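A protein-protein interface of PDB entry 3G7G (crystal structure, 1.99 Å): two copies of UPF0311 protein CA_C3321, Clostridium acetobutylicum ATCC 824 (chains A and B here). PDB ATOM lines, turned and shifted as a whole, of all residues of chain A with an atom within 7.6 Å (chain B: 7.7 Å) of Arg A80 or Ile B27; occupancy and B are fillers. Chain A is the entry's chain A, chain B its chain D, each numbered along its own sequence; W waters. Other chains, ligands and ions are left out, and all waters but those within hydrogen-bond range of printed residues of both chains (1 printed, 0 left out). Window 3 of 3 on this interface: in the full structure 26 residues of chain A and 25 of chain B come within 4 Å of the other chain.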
ATOM      1  N   GLY A  44      25.680   9.903  13.451  1.00  0.00           N
ATOM      2  CA  GLY A  44      26.181   9.401  12.203  1.00  0.00           C
ATOM      3  C   GLY A  44      25.227   9.664  11.072  1.00  0.00           C
ATOM      4  O   GLY A  44      23.989   9.626  11.230  1.00  0.00           O
ATOM      5  N   VAL A  46      24.068   8.598   7.250  1.00  0.00           N
ATOM      6  CA  VAL A  46      24.027   7.500   6.307  1.00  0.00           C
ATOM      7  C   VAL A  46      23.794   8.098   4.921  1.00  0.00           C
ATOM      8  O   VAL A  46      22.894   8.921   4.741  1.00  0.00           O
ATOM      9  CB  VAL A  46      22.891   6.513   6.636  1.00  0.00           C
ATOM     10  CG1 VAL A  46      22.876   5.362   5.629  1.00  0.00           C
ATOM     11  CG2 VAL A  46      22.982   6.032   8.081  1.00  0.00           C
ATOM     12  N   PHE A  51      19.672   5.651  -0.301  1.00  0.00           N
ATOM     13  CA  PHE A  51      19.945   5.102   1.007  1.00  0.00           C
ATOM     14  C   PHE A  51      20.512   6.197   1.885  1.00  0.00           C
ATOM     15  O   PHE A  51      21.718   6.238   2.098  1.00  0.00           O
ATOM     16  CB  PHE A  51      20.923   3.911   0.889  1.00  0.00           C
ATOM     17  CG  PHE A  51      20.753   2.892   1.957  1.00  0.00           C
ATOM     18  CD1 PHE A  51      19.992   1.752   1.731  1.00  0.00           C
ATOM     19  CD2 PHE A  51      21.354   3.071   3.202  1.00  0.00           C
ATOM     20  CE1 PHE A  51      19.814   0.817   2.724  1.00  0.00           C
ATOM     21  CE2 PHE A  51      21.200   2.112   4.228  1.00  0.00           C
ATOM     22  CZ  PHE A  51      20.427   0.990   3.993  1.00  0.00           C
ATOM     23  N   ASN A  52      19.634   7.072   2.392  1.00  0.00           N
ATOM     24  CA  ASN A  52      20.030   8.259   3.163  1.00  0.00           C
ATOM     25  C   ASN A  52      19.325   8.328   4.523  1.00  0.00           C
ATOM     26  O   ASN A  52      18.107   8.191   4.604  1.00  0.00           O
ATOM     27  CB  ASN A  52      19.768   9.514   2.315  1.00  0.00           C
ATOM     28  CG  ASN A  52      20.548   9.488   0.975  1.00  0.00           C
ATOM     29  OD1 ASN A  52      21.781   9.588   0.946  1.00  0.00           O
ATOM     30  ND2 ASN A  52      19.822   9.335  -0.128  1.00  0.00           N
ATOM     31  N   GLY A  53      20.082   8.476   5.610  1.00  0.00           N
ATOM     32  CA  GLY A  53      19.473   8.501   6.930  1.00  0.00           C
ATOM     33  C   GLY A  53      20.424   8.907   8.018  1.00  0.00           C
ATOM     34  O   GLY A  53      21.395   9.621   7.780  1.00  0.00           O
ATOM     35  N   LYS A  54      20.130   8.452   9.236  1.00  0.00           N
ATOM     36  CA  LYS A  54      20.915   8.808  10.393  1.00  0.00           C
ATOM     37  C   LYS A  54      21.074   7.581  11.287  1.00  0.00           C
ATOM     38  O   LYS A  54      20.284   6.644  11.216  1.00  0.00           O
ATOM     39  CB  LYS A  54      20.265   9.958  11.170  1.00  0.00           C
ATOM     40  CG  LYS A  54      19.028   9.526  11.976  1.00  0.00           C
ATOM     41  CD  LYS A  54      18.116  10.693  12.413  1.00  0.00           C
ATOM     42  CE  LYS A  54      18.756  11.577  13.518  1.00  0.00           C
ATOM     43  NZ  LYS A  54      18.014  12.935  13.647  1.00  0.00           N
ATOM     44  N   VAL A  55      22.124   7.595  12.093  1.00  0.00           N
ATOM     45  CA  VAL A  55      22.307   6.629  13.165  1.00  0.00           C
ATOM     46  C   VAL A  55      21.420   6.999  14.346  1.00  0.00           C
ATOM     47  O   VAL A  55      21.289   8.164  14.683  1.00  0.00           O
ATOM     48  CB  VAL A  55      23.757   6.617  13.610  1.00  0.00           C
ATOM     49  CG1 VAL A  55      23.949   5.723  14.775  1.00  0.00           C
ATOM     50  CG2 VAL A  55      24.678   6.191  12.419  1.00  0.00           C
ATOM     51  N   LEU A  56      20.818   5.993  14.980  1.00  0.00           N
ATOM     52  CA  LEU A  56      19.914   6.207  16.129  1.00  0.00           C
ATOM     53  C   LEU A  56      20.696   6.142  17.459  1.00  0.00           C
ATOM     54  O   LEU A  56      21.864   5.782  17.466  1.00  0.00           O
ATOM     55  CB  LEU A  56      18.806   5.150  16.096  1.00  0.00           C
ATOM     56  CG  LEU A  56      17.795   5.195  14.956  1.00  0.00           C
ATOM     57  CD1 LEU A  56      16.847   3.962  14.939  1.00  0.00           C
ATOM     58  CD2 LEU A  56      16.976   6.509  15.031  1.00  0.00           C
ATOM     59  N   PRO A  57      20.069   6.518  18.587  1.00  0.00           N
ATOM     60  CA  PRO A  57      20.762   6.369  19.888  1.00  0.00           C
ATOM     61  C   PRO A  57      21.013   4.908  20.256  1.00  0.00           C
ATOM     62  O   PRO A  57      20.388   4.011  19.703  1.00  0.00           O
ATOM     63  CB  PRO A  57      19.783   6.998  20.884  1.00  0.00           C
ATOM     64  CG  PRO A  57      18.818   7.865  20.015  1.00  0.00           C
ATOM     65  CD  PRO A  57      18.721   7.100  18.745  1.00  0.00           C
ATOM     66  N   GLY A  58      21.939   4.677  21.164  1.00  0.00           N
ATOM     67  CA  GLY A  58      22.142   3.339  21.731  1.00  0.00           C
ATOM     68  C   GLY A  58      23.346   2.572  21.232  1.00  0.00           C
ATOM     69  O   GLY A  58      23.570   1.463  21.663  1.00  0.00           O
ATOM     70  N   TYR A  77      24.485  -1.074  16.644  1.00  0.00           N
ATOM     71  CA  TYR A  77      23.780   0.180  16.496  1.00  0.00           C
ATOM     72  C   TYR A  77      22.734   0.052  15.391  1.00  0.00           C
ATOM     73  O   TYR A  77      22.596  -1.008  14.782  1.00  0.00           O
ATOM     74  CB  TYR A  77      24.776   1.298  16.202  1.00  0.00           C
ATOM     75  CG  TYR A  77      25.608   1.117  14.957  1.00  0.00           C
ATOM     76  CD1 TYR A  77      25.258   1.733  13.764  1.00  0.00           C
ATOM     77  CD2 TYR A  77      26.774   0.379  14.985  1.00  0.00           C
ATOM     78  CE1 TYR A  77      26.043   1.575  12.630  1.00  0.00           C
ATOM     79  CE2 TYR A  77      27.541   0.195  13.852  1.00  0.00           C
ATOM     80  CZ  TYR A  77      27.184   0.803  12.680  1.00  0.00           C
ATOM     81  OH  TYR A  77      27.983   0.630  11.556  1.00  0.00           O
ATOM     82  N   ALA A  78      22.005   1.136  15.107  1.00  0.00           N
ATOM     83  CA  ALA A  78      20.857   1.103  14.218  1.00  0.00           C
ATOM     84  C   ALA A  78      20.792   2.410  13.471  1.00  0.00           C
ATOM     85  O   ALA A  78      21.312   3.445  13.916  1.00  0.00           O
ATOM     86  CB  ALA A  78      19.569   0.901  14.999  1.00  0.00           C
ATOM     87  N   ILE A  79      20.184   2.340  12.311  1.00  0.00           N
ATOM     88  CA  ILE A  79      20.016   3.519  11.501  1.00  0.00           C
ATOM     89  C   ILE A  79      18.549   3.620  11.176  1.00  0.00           C
ATOM     90  O   ILE A  79      17.828   2.630  11.205  1.00  0.00           O
ATOM     91  CB  ILE A  79      20.883   3.510  10.232  1.00  0.00           C
ATOM     92  CG1 ILE A  79      20.636   2.315   9.334  1.00  0.00           C
ATOM     93  CG2 ILE A  79      22.363   3.434  10.574  1.00  0.00           C
ATOM     94  CD1 ILE A  79      21.573   2.333   8.139  1.00  0.00           C
ATOM     95  N   ARG A  80      18.117   4.841  10.908  1.00  0.00           N
ATOM     96  CA  ARG A  80      16.794   5.139  10.472  1.00  0.00           C
ATOM     97  C   ARG A  80      16.919   5.853   9.159  1.00  0.00           C
ATOM     98  O   ARG A  80      17.569   6.887   9.089  1.00  0.00           O
ATOM     99  CB  ARG A  80      16.137   6.065  11.453  1.00  0.00           C
ATOM    100  CG  ARG A  80      14.763   6.538  10.995  1.00  0.00           C
ATOM    101  CD  ARG A  80      13.788   6.381  12.089  1.00  0.00           C
ATOM    102  NE  ARG A  80      13.063   5.160  11.866  1.00  0.00           N
ATOM    103  CZ  ARG A  80      12.769   4.267  12.790  1.00  0.00           C
ATOM    104  NH1 ARG A  80      13.200   4.382  14.047  1.00  0.00           N
ATOM    105  NH2 ARG A  80      12.089   3.208  12.424  1.00  0.00           N
ATOM    106  N   LEU A  81      16.278   5.308   8.134  1.00  0.00           N
ATOM    107  CA  LEU A  81      16.260   5.933   6.844  1.00  0.00           C
ATOM    108  C   LEU A  81      15.150   6.975   6.732  1.00  0.00           C
ATOM    109  O   LEU A  81      14.189   6.973   7.494  1.00  0.00           O
ATOM    110  CB  LEU A  81      16.110   4.889   5.750  1.00  0.00           C
ATOM    111  CG  LEU A  81      17.209   3.842   5.665  1.00  0.00           C
ATOM    112  CD1 LEU A  81      17.095   3.117   4.318  1.00  0.00           C
ATOM    113  CD2 LEU A  81      18.561   4.508   5.806  1.00  0.00           C
ATOM    114  N   ASP A  82      15.298   7.830   5.736  1.00  0.00           N
ATOM    115  CA  ASP A  82      14.413   8.941   5.523  1.00  0.00           C
ATOM    116  C   ASP A  82      12.997   8.513   5.089  1.00  0.00           C
ATOM    117  O   ASP A  82      12.087   9.289   5.209  1.00  0.00           O
ATOM    118  CB  ASP A  82      15.024   9.899   4.493  1.00  0.00           C
ATOM    119  CG  ASP A  82      15.246   9.241   3.144  1.00  0.00           C
ATOM    120  OD1 ASP A  82      15.121   7.979   3.071  1.00  0.00           O
ATOM    121  OD2 ASP A  82      15.560   9.983   2.174  1.00  0.00           O
ATOM    122  N   ASP A  83      12.822   7.290   4.598  1.00  0.00           N
ATOM    123  CA  ASP A  83      11.492   6.745   4.344  1.00  0.00           C
ATOM    124  C   ASP A  83      10.883   6.108   5.598  1.00  0.00           C
ATOM    125  O   ASP A  83       9.834   5.511   5.521  1.00  0.00           O
ATOM    126  CB  ASP A  83      11.526   5.724   3.198  1.00  0.00           C
ATOM    127  CG  ASP A  83      12.237   4.404   3.568  1.00  0.00           C
ATOM    128  OD1 ASP A  83      12.776   4.249   4.702  1.00  0.00           O
ATOM    129  OD2 ASP A  83      12.257   3.517   2.698  1.00  0.00           O
ATOM    130  N   GLY A  84      11.562   6.222   6.734  1.00  0.00           N
ATOM    131  CA  GLY A  84      11.071   5.726   8.016  1.00  0.00           C
ATOM    132  C   GLY A  84      11.500   4.318   8.435  1.00  0.00           C
ATOM    133  O   GLY A  84      11.261   3.926   9.580  1.00  0.00           O
ATOM    134  N   ALA A  85      12.114   3.560   7.535  1.00  0.00           N
ATOM    135  CA  ALA A  85      12.595   2.182   7.817  1.00  0.00           C
ATOM    136  C   ALA A  85      13.810   2.181   8.726  1.00  0.00           C
ATOM    137  O   ALA A  85      14.624   3.079   8.665  1.00  0.00           O
ATOM    138  CB  ALA A  85      12.953   1.480   6.520  1.00  0.00           C
ATOM    139  N   ALA A  86      13.921   1.169   9.580  1.00  0.00           N
ATOM    140  CA  ALA A  86      15.076   1.001  10.430  1.00  0.00           C
ATOM    141  C   ALA A  86      15.888  -0.197   9.989  1.00  0.00           C
ATOM    142  O   ALA A  86      15.372  -1.135   9.392  1.00  0.00           O
ATOM    143  CB  ALA A  86      14.641   0.821  11.886  1.00  0.00           C
ATOM    144  N   ILE A  87      17.178  -0.151  10.307  1.00  0.00           N
ATOM    145  CA  ILE A  87      18.103  -1.263  10.118  1.00  0.00           C
ATOM    146  C   ILE A  87      18.974  -1.344  11.341  1.00  0.00           C
ATOM    147  O   ILE A  87      19.594  -0.371  11.720  1.00  0.00           O
ATOM    148  CB  ILE A  87      19.023  -1.050   8.882  1.00  0.00           C
ATOM    149  CG1 ILE A  87      18.179  -0.809   7.622  1.00  0.00           C
ATOM    150  CG2 ILE A  87      19.935  -2.297   8.652  1.00  0.00           C
ATOM    151  CD1 ILE A  87      18.446   0.436   6.904  1.00  0.00           C
ATOM    152  N   TYR A  88      19.016  -2.533  11.927  1.00  0.00           N
ATOM    153  CA  TYR A  88      19.846  -2.861  13.051  1.00  0.00           C
ATOM    154  C   TYR A  88      21.098  -3.570  12.534  1.00  0.00           C
ATOM    155  O   TYR A  88      21.021  -4.532  11.748  1.00  0.00           O
ATOM    156  CB  TYR A  88      19.065  -3.751  13.996  1.00  0.00           C
ATOM    157  CG  TYR A  88      19.895  -4.280  15.101  1.00  0.00           C
ATOM    158  CD1 TYR A  88      20.459  -3.418  16.049  1.00  0.00           C
ATOM    159  CD2 TYR A  88      20.142  -5.639  15.211  1.00  0.00           C
ATOM    160  CE1 TYR A  88      21.259  -3.909  17.082  1.00  0.00           C
ATOM    161  CE2 TYR A  88      20.914  -6.132  16.243  1.00  0.00           C
ATOM    162  CZ  TYR A  88      21.483  -5.262  17.163  1.00  0.00           C
ATOM    163  OH  TYR A  88      22.242  -5.764  18.189  1.00  0.00           O
ATOM    164  N   ILE A  89      22.246  -3.087  12.968  1.00  0.00           N
ATOM    165  CA  ILE A  89      23.534  -3.494  12.420  1.00  0.00           C
ATOM    166  C   ILE A  89      24.380  -4.089  13.527  1.00  0.00           C
ATOM    167  O   ILE A  89      24.493  -3.479  14.567  1.00  0.00           O
ATOM    168  CB  ILE A  89      24.306  -2.273  11.862  1.00  0.00           C
ATOM    169  CG1 ILE A  89      23.433  -1.523  10.885  1.00  0.00           C
ATOM    170  CG2 ILE A  89      25.641  -2.688  11.180  1.00  0.00           C
ATOM    171  CD1 ILE A  89      24.145  -0.526  10.091  1.00  0.00           C
ATOM    172  N   GLU A 125      19.539  -6.508  10.267  1.00  0.00           N
ATOM    173  CA  GLU A 125      18.190  -6.924  10.613  1.00  0.00           C
ATOM    174  C   GLU A 125      17.250  -5.813  10.172  1.00  0.00           C
ATOM    175  O   GLU A 125      17.467  -4.688  10.517  1.00  0.00           O
ATOM    176  CB  GLU A 125      18.114  -7.204  12.101  1.00  0.00           C
ATOM    177  CG  GLU A 125      16.783  -7.629  12.564  1.00  0.00           C
ATOM    178  CD  GLU A 125      16.745  -7.856  14.002  1.00  0.00           C
ATOM    179  OE1 GLU A 125      16.377  -6.930  14.731  1.00  0.00           O
ATOM    180  OE2 GLU A 125      17.089  -8.965  14.416  1.00  0.00           O
ATOM    181  N   TYR A 127      12.934  -4.717   8.752  1.00  0.00           N
ATOM    182  CA  TYR A 127      11.528  -4.961   9.166  1.00  0.00           C
ATOM    183  C   TYR A 127      10.526  -4.585   8.088  1.00  0.00           C
ATOM    184  O   TYR A 127       9.352  -4.247   8.365  1.00  0.00           O
ATOM    185  CB  TYR A 127      11.214  -4.216  10.478  1.00  0.00           C
ATOM    186  CG  TYR A 127      12.395  -4.258  11.399  1.00  0.00           C
ATOM    187  CD1 TYR A 127      12.566  -5.311  12.279  1.00  0.00           C
ATOM    188  CD2 TYR A 127      13.396  -3.289  11.327  1.00  0.00           C
ATOM    189  CE1 TYR A 127      13.684  -5.385  13.091  1.00  0.00           C
ATOM    190  CE2 TYR A 127      14.506  -3.347  12.155  1.00  0.00           C
ATOM    191  CZ  TYR A 127      14.656  -4.422  13.020  1.00  0.00           C
ATOM    192  OH  TYR A 127      15.761  -4.513  13.866  1.00  0.00           O
ATOM    193  N   PRO B  24      13.321   1.930  26.552  1.00  0.00           N
ATOM    194  CA  PRO B  24      13.868   1.248  25.373  1.00  0.00           C
ATOM    195  C   PRO B  24      13.998   2.166  24.178  1.00  0.00           C
ATOM    196  O   PRO B  24      13.192   3.060  24.017  1.00  0.00           O
ATOM    197  CB  PRO B  24      12.827   0.180  25.048  1.00  0.00           C
ATOM    198  CG  PRO B  24      12.004   0.025  26.299  1.00  0.00           C
ATOM    199  CD  PRO B  24      12.021   1.367  26.952  1.00  0.00           C
ATOM    200  N   ILE B  25      15.015   1.931  23.363  1.00  0.00           N
ATOM    201  CA  ILE B  25      15.159   2.597  22.091  1.00  0.00           C
ATOM    202  C   ILE B  25      14.592   1.610  21.111  1.00  0.00           C
ATOM    203  O   ILE B  25      15.275   0.668  20.726  1.00  0.00           O
ATOM    204  CB  ILE B  25      16.632   2.886  21.767  1.00  0.00           C
ATOM    205  CG1 ILE B  25      17.244   3.769  22.840  1.00  0.00           C
ATOM    206  CG2 ILE B  25      16.765   3.586  20.428  1.00  0.00           C
ATOM    207  CD1 ILE B  25      18.763   3.961  22.672  1.00  0.00           C
ATOM    208  N   LEU B  26      13.329   1.792  20.740  1.00  0.00           N
ATOM    209  CA  LEU B  26      12.681   0.941  19.735  1.00  0.00           C
ATOM    210  C   LEU B  26      13.297   1.141  18.348  1.00  0.00           C
ATOM    211  O   LEU B  26      13.289   2.239  17.816  1.00  0.00           O
ATOM    212  CB  LEU B  26      11.172   1.178  19.687  1.00  0.00           C
ATOM    213  CG  LEU B  26      10.347   0.184  18.810  1.00  0.00           C
ATOM    214  CD1 LEU B  26      10.651  -1.275  19.140  1.00  0.00           C
ATOM    215  CD2 LEU B  26       8.812   0.423  18.972  1.00  0.00           C
ATOM    216  N   ILE B  27      13.820   0.064  17.776  1.00  0.00           N
ATOM    217  CA  ILE B  27      14.455   0.089  16.479  1.00  0.00           C
ATOM    218  C   ILE B  27      13.406  -0.239  15.409  1.00  0.00           C
ATOM    219  O   ILE B  27      13.131   0.585  14.548  1.00  0.00           O
ATOM    220  CB  ILE B  27      15.641  -0.896  16.406  1.00  0.00           C
ATOM    221  CG1 ILE B  27      16.636  -0.638  17.572  1.00  0.00           C
ATOM    222  CG2 ILE B  27      16.328  -0.837  15.013  1.00  0.00           C
ATOM    223  CD1 ILE B  27      17.053   0.836  17.691  1.00  0.00           C
ATOM    224  N   GLY B  28      12.791  -1.418  15.485  1.00  0.00           N
ATOM    225  CA  GLY B  28      11.783  -1.784  14.521  1.00  0.00           C
ATOM    226  C   GLY B  28      11.097  -3.051  14.885  1.00  0.00           C
ATOM    227  O   GLY B  28      11.558  -3.747  15.776  1.00  0.00           O
ATOM    228  N   GLN B  29      10.013  -3.372  14.181  1.00  0.00           N
ATOM    229  CA  GLN B  29       9.306  -4.644  14.417  1.00  0.00           C
ATOM    230  C   GLN B  29       8.644  -5.128  13.130  1.00  0.00           C
ATOM    231  O   GLN B  29       8.237  -4.318  12.292  1.00  0.00           O
ATOM    232  CB  GLN B  29       8.217  -4.436  15.495  1.00  0.00           C
ATOM    233  CG  GLN B  29       7.245  -5.575  15.699  1.00  0.00           C
ATOM    234  CD  GLN B  29       6.208  -5.305  16.807  1.00  0.00           C
ATOM    235  OE1 GLN B  29       6.502  -4.615  17.779  1.00  0.00           O
ATOM    236  NE2 GLN B  29       4.979  -5.827  16.632  1.00  0.00           N
ATOM    237  N   ARG B  35      10.379  -7.839  17.421  1.00  0.00           N
ATOM    238  CA  ARG B  35      10.580  -6.464  17.862  1.00  0.00           C
ATOM    239  C   ARG B  35      11.959  -6.234  18.491  1.00  0.00           C
ATOM    240  O   ARG B  35      12.238  -6.727  19.591  1.00  0.00           O
ATOM    241  CB  ARG B  35       9.523  -6.058  18.904  1.00  0.00           C
ATOM    242  CG  ARG B  35       9.806  -4.663  19.516  1.00  0.00           C
ATOM    243  CD  ARG B  35       8.615  -4.017  20.208  1.00  0.00           C
ATOM    244  NE  ARG B  35       7.856  -4.975  20.996  1.00  0.00           N
ATOM    245  CZ  ARG B  35       8.030  -5.237  22.296  1.00  0.00           C
ATOM    246  NH1 ARG B  35       8.962  -4.603  23.007  1.00  0.00           N
ATOM    247  NH2 ARG B  35       7.243  -6.140  22.893  1.00  0.00           N
ATOM    248  N   ARG B  36      12.785  -5.472  17.792  1.00  0.00           N
ATOM    249  CA  ARG B  36      14.131  -5.103  18.233  1.00  0.00           C
ATOM    250  C   ARG B  36      14.161  -3.779  18.994  1.00  0.00           C
ATOM    251  O   ARG B  36      13.744  -2.734  18.486  1.00  0.00           O
ATOM    252  CB  ARG B  36      15.059  -4.989  17.001  1.00  0.00           C
ATOM    253  CG  ARG B  36      16.558  -4.549  17.263  1.00  0.00           C
ATOM    254  CD  ARG B  36      17.391  -5.529  18.088  1.00  0.00           C
ATOM    255  NE  ARG B  36      17.505  -6.822  17.391  1.00  0.00           N
ATOM    256  CZ  ARG B  36      18.163  -7.883  17.845  1.00  0.00           C
ATOM    257  NH1 ARG B  36      18.759  -7.853  19.017  1.00  0.00           N
ATOM    258  NH2 ARG B  36      18.205  -8.999  17.145  1.00  0.00           N
ATOM    259  N   GLN B  37      14.750  -3.817  20.182  1.00  0.00           N
ATOM    260  CA  GLN B  37      15.007  -2.608  20.948  1.00  0.00           C
ATOM    261  C   GLN B  37      16.344  -2.668  21.717  1.00  0.00           C
ATOM    262  O   GLN B  37      16.826  -3.739  22.090  1.00  0.00           O
ATOM    263  CB  GLN B  37      13.853  -2.363  21.925  1.00  0.00           C
ATOM    264  CG  GLN B  37      13.749  -3.433  22.953  1.00  0.00           C
ATOM    265  CD  GLN B  37      12.350  -3.581  23.583  1.00  0.00           C
ATOM    266  OE1 GLN B  37      11.472  -2.730  23.420  1.00  0.00           O
ATOM    267  NE2 GLN B  37      12.160  -4.692  24.334  1.00  0.00           N
ATOM    268  N   LEU B  38      16.924  -1.490  21.918  1.00  0.00           N
ATOM    269  CA  LEU B  38      18.149  -1.331  22.695  1.00  0.00           C
ATOM    270  C   LEU B  38      17.794  -0.652  24.027  1.00  0.00           C
ATOM    271  O   LEU B  38      17.113   0.397  24.062  1.00  0.00           O
ATOM    272  CB  LEU B  38      19.183  -0.528  21.917  1.00  0.00           C
ATOM    273  CG  LEU B  38      19.552  -1.048  20.522  1.00  0.00           C
ATOM    274  CD1 LEU B  38      20.465  -0.032  19.736  1.00  0.00           C
ATOM    275  CD2 LEU B  38      20.169  -2.459  20.588  1.00  0.00           C
ATOM    276  N   SER B  62      20.756  -5.430  24.044  1.00  0.00           N
ATOM    277  CA  SER B  62      20.112  -5.588  22.770  1.00  0.00           C
ATOM    278  C   SER B  62      19.142  -6.782  22.863  1.00  0.00           C
ATOM    279  O   SER B  62      19.545  -7.918  23.157  1.00  0.00           O
ATOM    280  CB  SER B  62      21.141  -5.789  21.674  1.00  0.00           C
ATOM    281  OG  SER B  62      20.532  -5.782  20.419  1.00  0.00           O
ATOM    282  N   GLN B  63      17.871  -6.486  22.619  1.00  0.00           N
ATOM    283  CA  GLN B  63      16.756  -7.397  22.825  1.00  0.00           C
ATOM    284  C   GLN B  63      15.917  -7.590  21.600  1.00  0.00           C
ATOM    285  O   GLN B  63      15.681  -6.664  20.866  1.00  0.00           O
ATOM    286  CB  GLN B  63      15.831  -6.821  23.864  1.00  0.00           C
ATOM    287  CG  GLN B  63      16.534  -6.496  25.127  1.00  0.00           C
ATOM    288  CD  GLN B  63      15.588  -6.290  26.266  1.00  0.00           C
ATOM    289  OE1 GLN B  63      14.413  -5.906  26.075  1.00  0.00           O
ATOM    290  NE2 GLN B  63      16.082  -6.545  27.466  1.00  0.00           N
HETATM  291  O   HOH W   1      11.104   1.002  12.889  1.00  0.00           O
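Among the printed residues, merely in contact across the chains: Ala A86 with Ile B27 (3.1 Å), Tyr A127 with Arg B36 (3.2 Å), Pro A57 with Ile B25 (3.4 Å), Tyr A127 with Gln B29 (3.5 Å), Arg A80 with Ile B27 (3.5 Å), Gly A58 with Ile B25 (3.6 Å), Tyr A88 with Arg B36 (3.6 Å), Ala A78 with Ile B27 (3.7 Å), Tyr A127 with Gly B28 (3.7 Å), Tyr A127 with Ile B27 (3.9 Å), Tyr A88 with Leu B38 (3.9 Å) and Gly A58 with Leu B38 (3.9 Å).
Of the printed residues of chain B, Gly A58 touches Ile B25 (3.6 Å) and Leu B38 (3.9 Å).
Arg A80 touches just one residue of chain B: Ile B27 (3.5 Å).
Ile A87 touches none of the printed residues of chain B.
Printed residues of chain A within 4 Å of Ile B25: Pro A57 and Gly A58.
Of chain A, only Ala A78, Arg A80, Ala A86 and Tyr A127 come within 4 Å of Ile B27.
The nearest residue of chain A that does not touch Ile B27 is Tyr A88 (4.1 Å).
The nearest printed residue of chain A that does not touch Ile B25 is Leu A56 (5.0 Å).
Of the 12 printed residues of chain B, 7 touch a printed residue of chain A.
Printed residues of chain A that touch a printed residue of chain B: Pro A57, Gly A58, Ala A78, Arg A80, Ala A86, Tyr A88, Glu A125 and Tyr A127.
Hydrophobic or aromatic side chains of chain A within 4 Å of the printed part of chain B: Pro A57, Ala A78, Ala A86, Tyr A88 and Tyr A127.
Along chain A the printed residues that touch a printed residue of chain B span positions 57 to 127.
Among the printed residues, Asp or Glu carboxylates within 4 Å of a Lys or Arg side-chain nitrogen of the other chain: Glu A125 with Arg B36 (2.9 Å).
OE1 of Glu A125 is in salt-bridge range of NE of Arg B36 (2.9 Å).
The side-chain hydroxyl (OH) of Tyr A88 sits at hydrogen-bond distance from the side-chain hydroxyl (OG) of Ser B62, at 2.8 Å.
No position is printed for both chains.
Of the 14 pairs that touch across the chains among the printed residues, none has its exchanged pair printed and touching as well.
NH1 of Arg B36 lies within hydrogen-bond range of OG of Ser B62 (3.1 Å).
OE1 of Glu A125 lies within hydrogen-bond range of OH of Tyr A127.
The backbone carbonyl oxygen (O) of Tyr A88 is in hydrogen-bond range of the backbone NH (N) of Glu A125, at 2.9 Å.
The backbone NH of Ile B25 sits at hydrogen-bond distance from the backbone carbonyl oxygen of Leu B38 (2.7 Å).
The backbone NH (N) of Ile B27 is in hydrogen-bond range of the backbone carbonyl oxygen (O) of Arg B36 (2.9 Å).
The guanidinium group of Arg A80 sits at hydrogen-bond distance from the backbone carbonyl oxygen of Gly A84, 3.0 Å away.
Water W1 lies within hydrogen-bond range of NH2 of Arg A80 and O of Ile B27.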
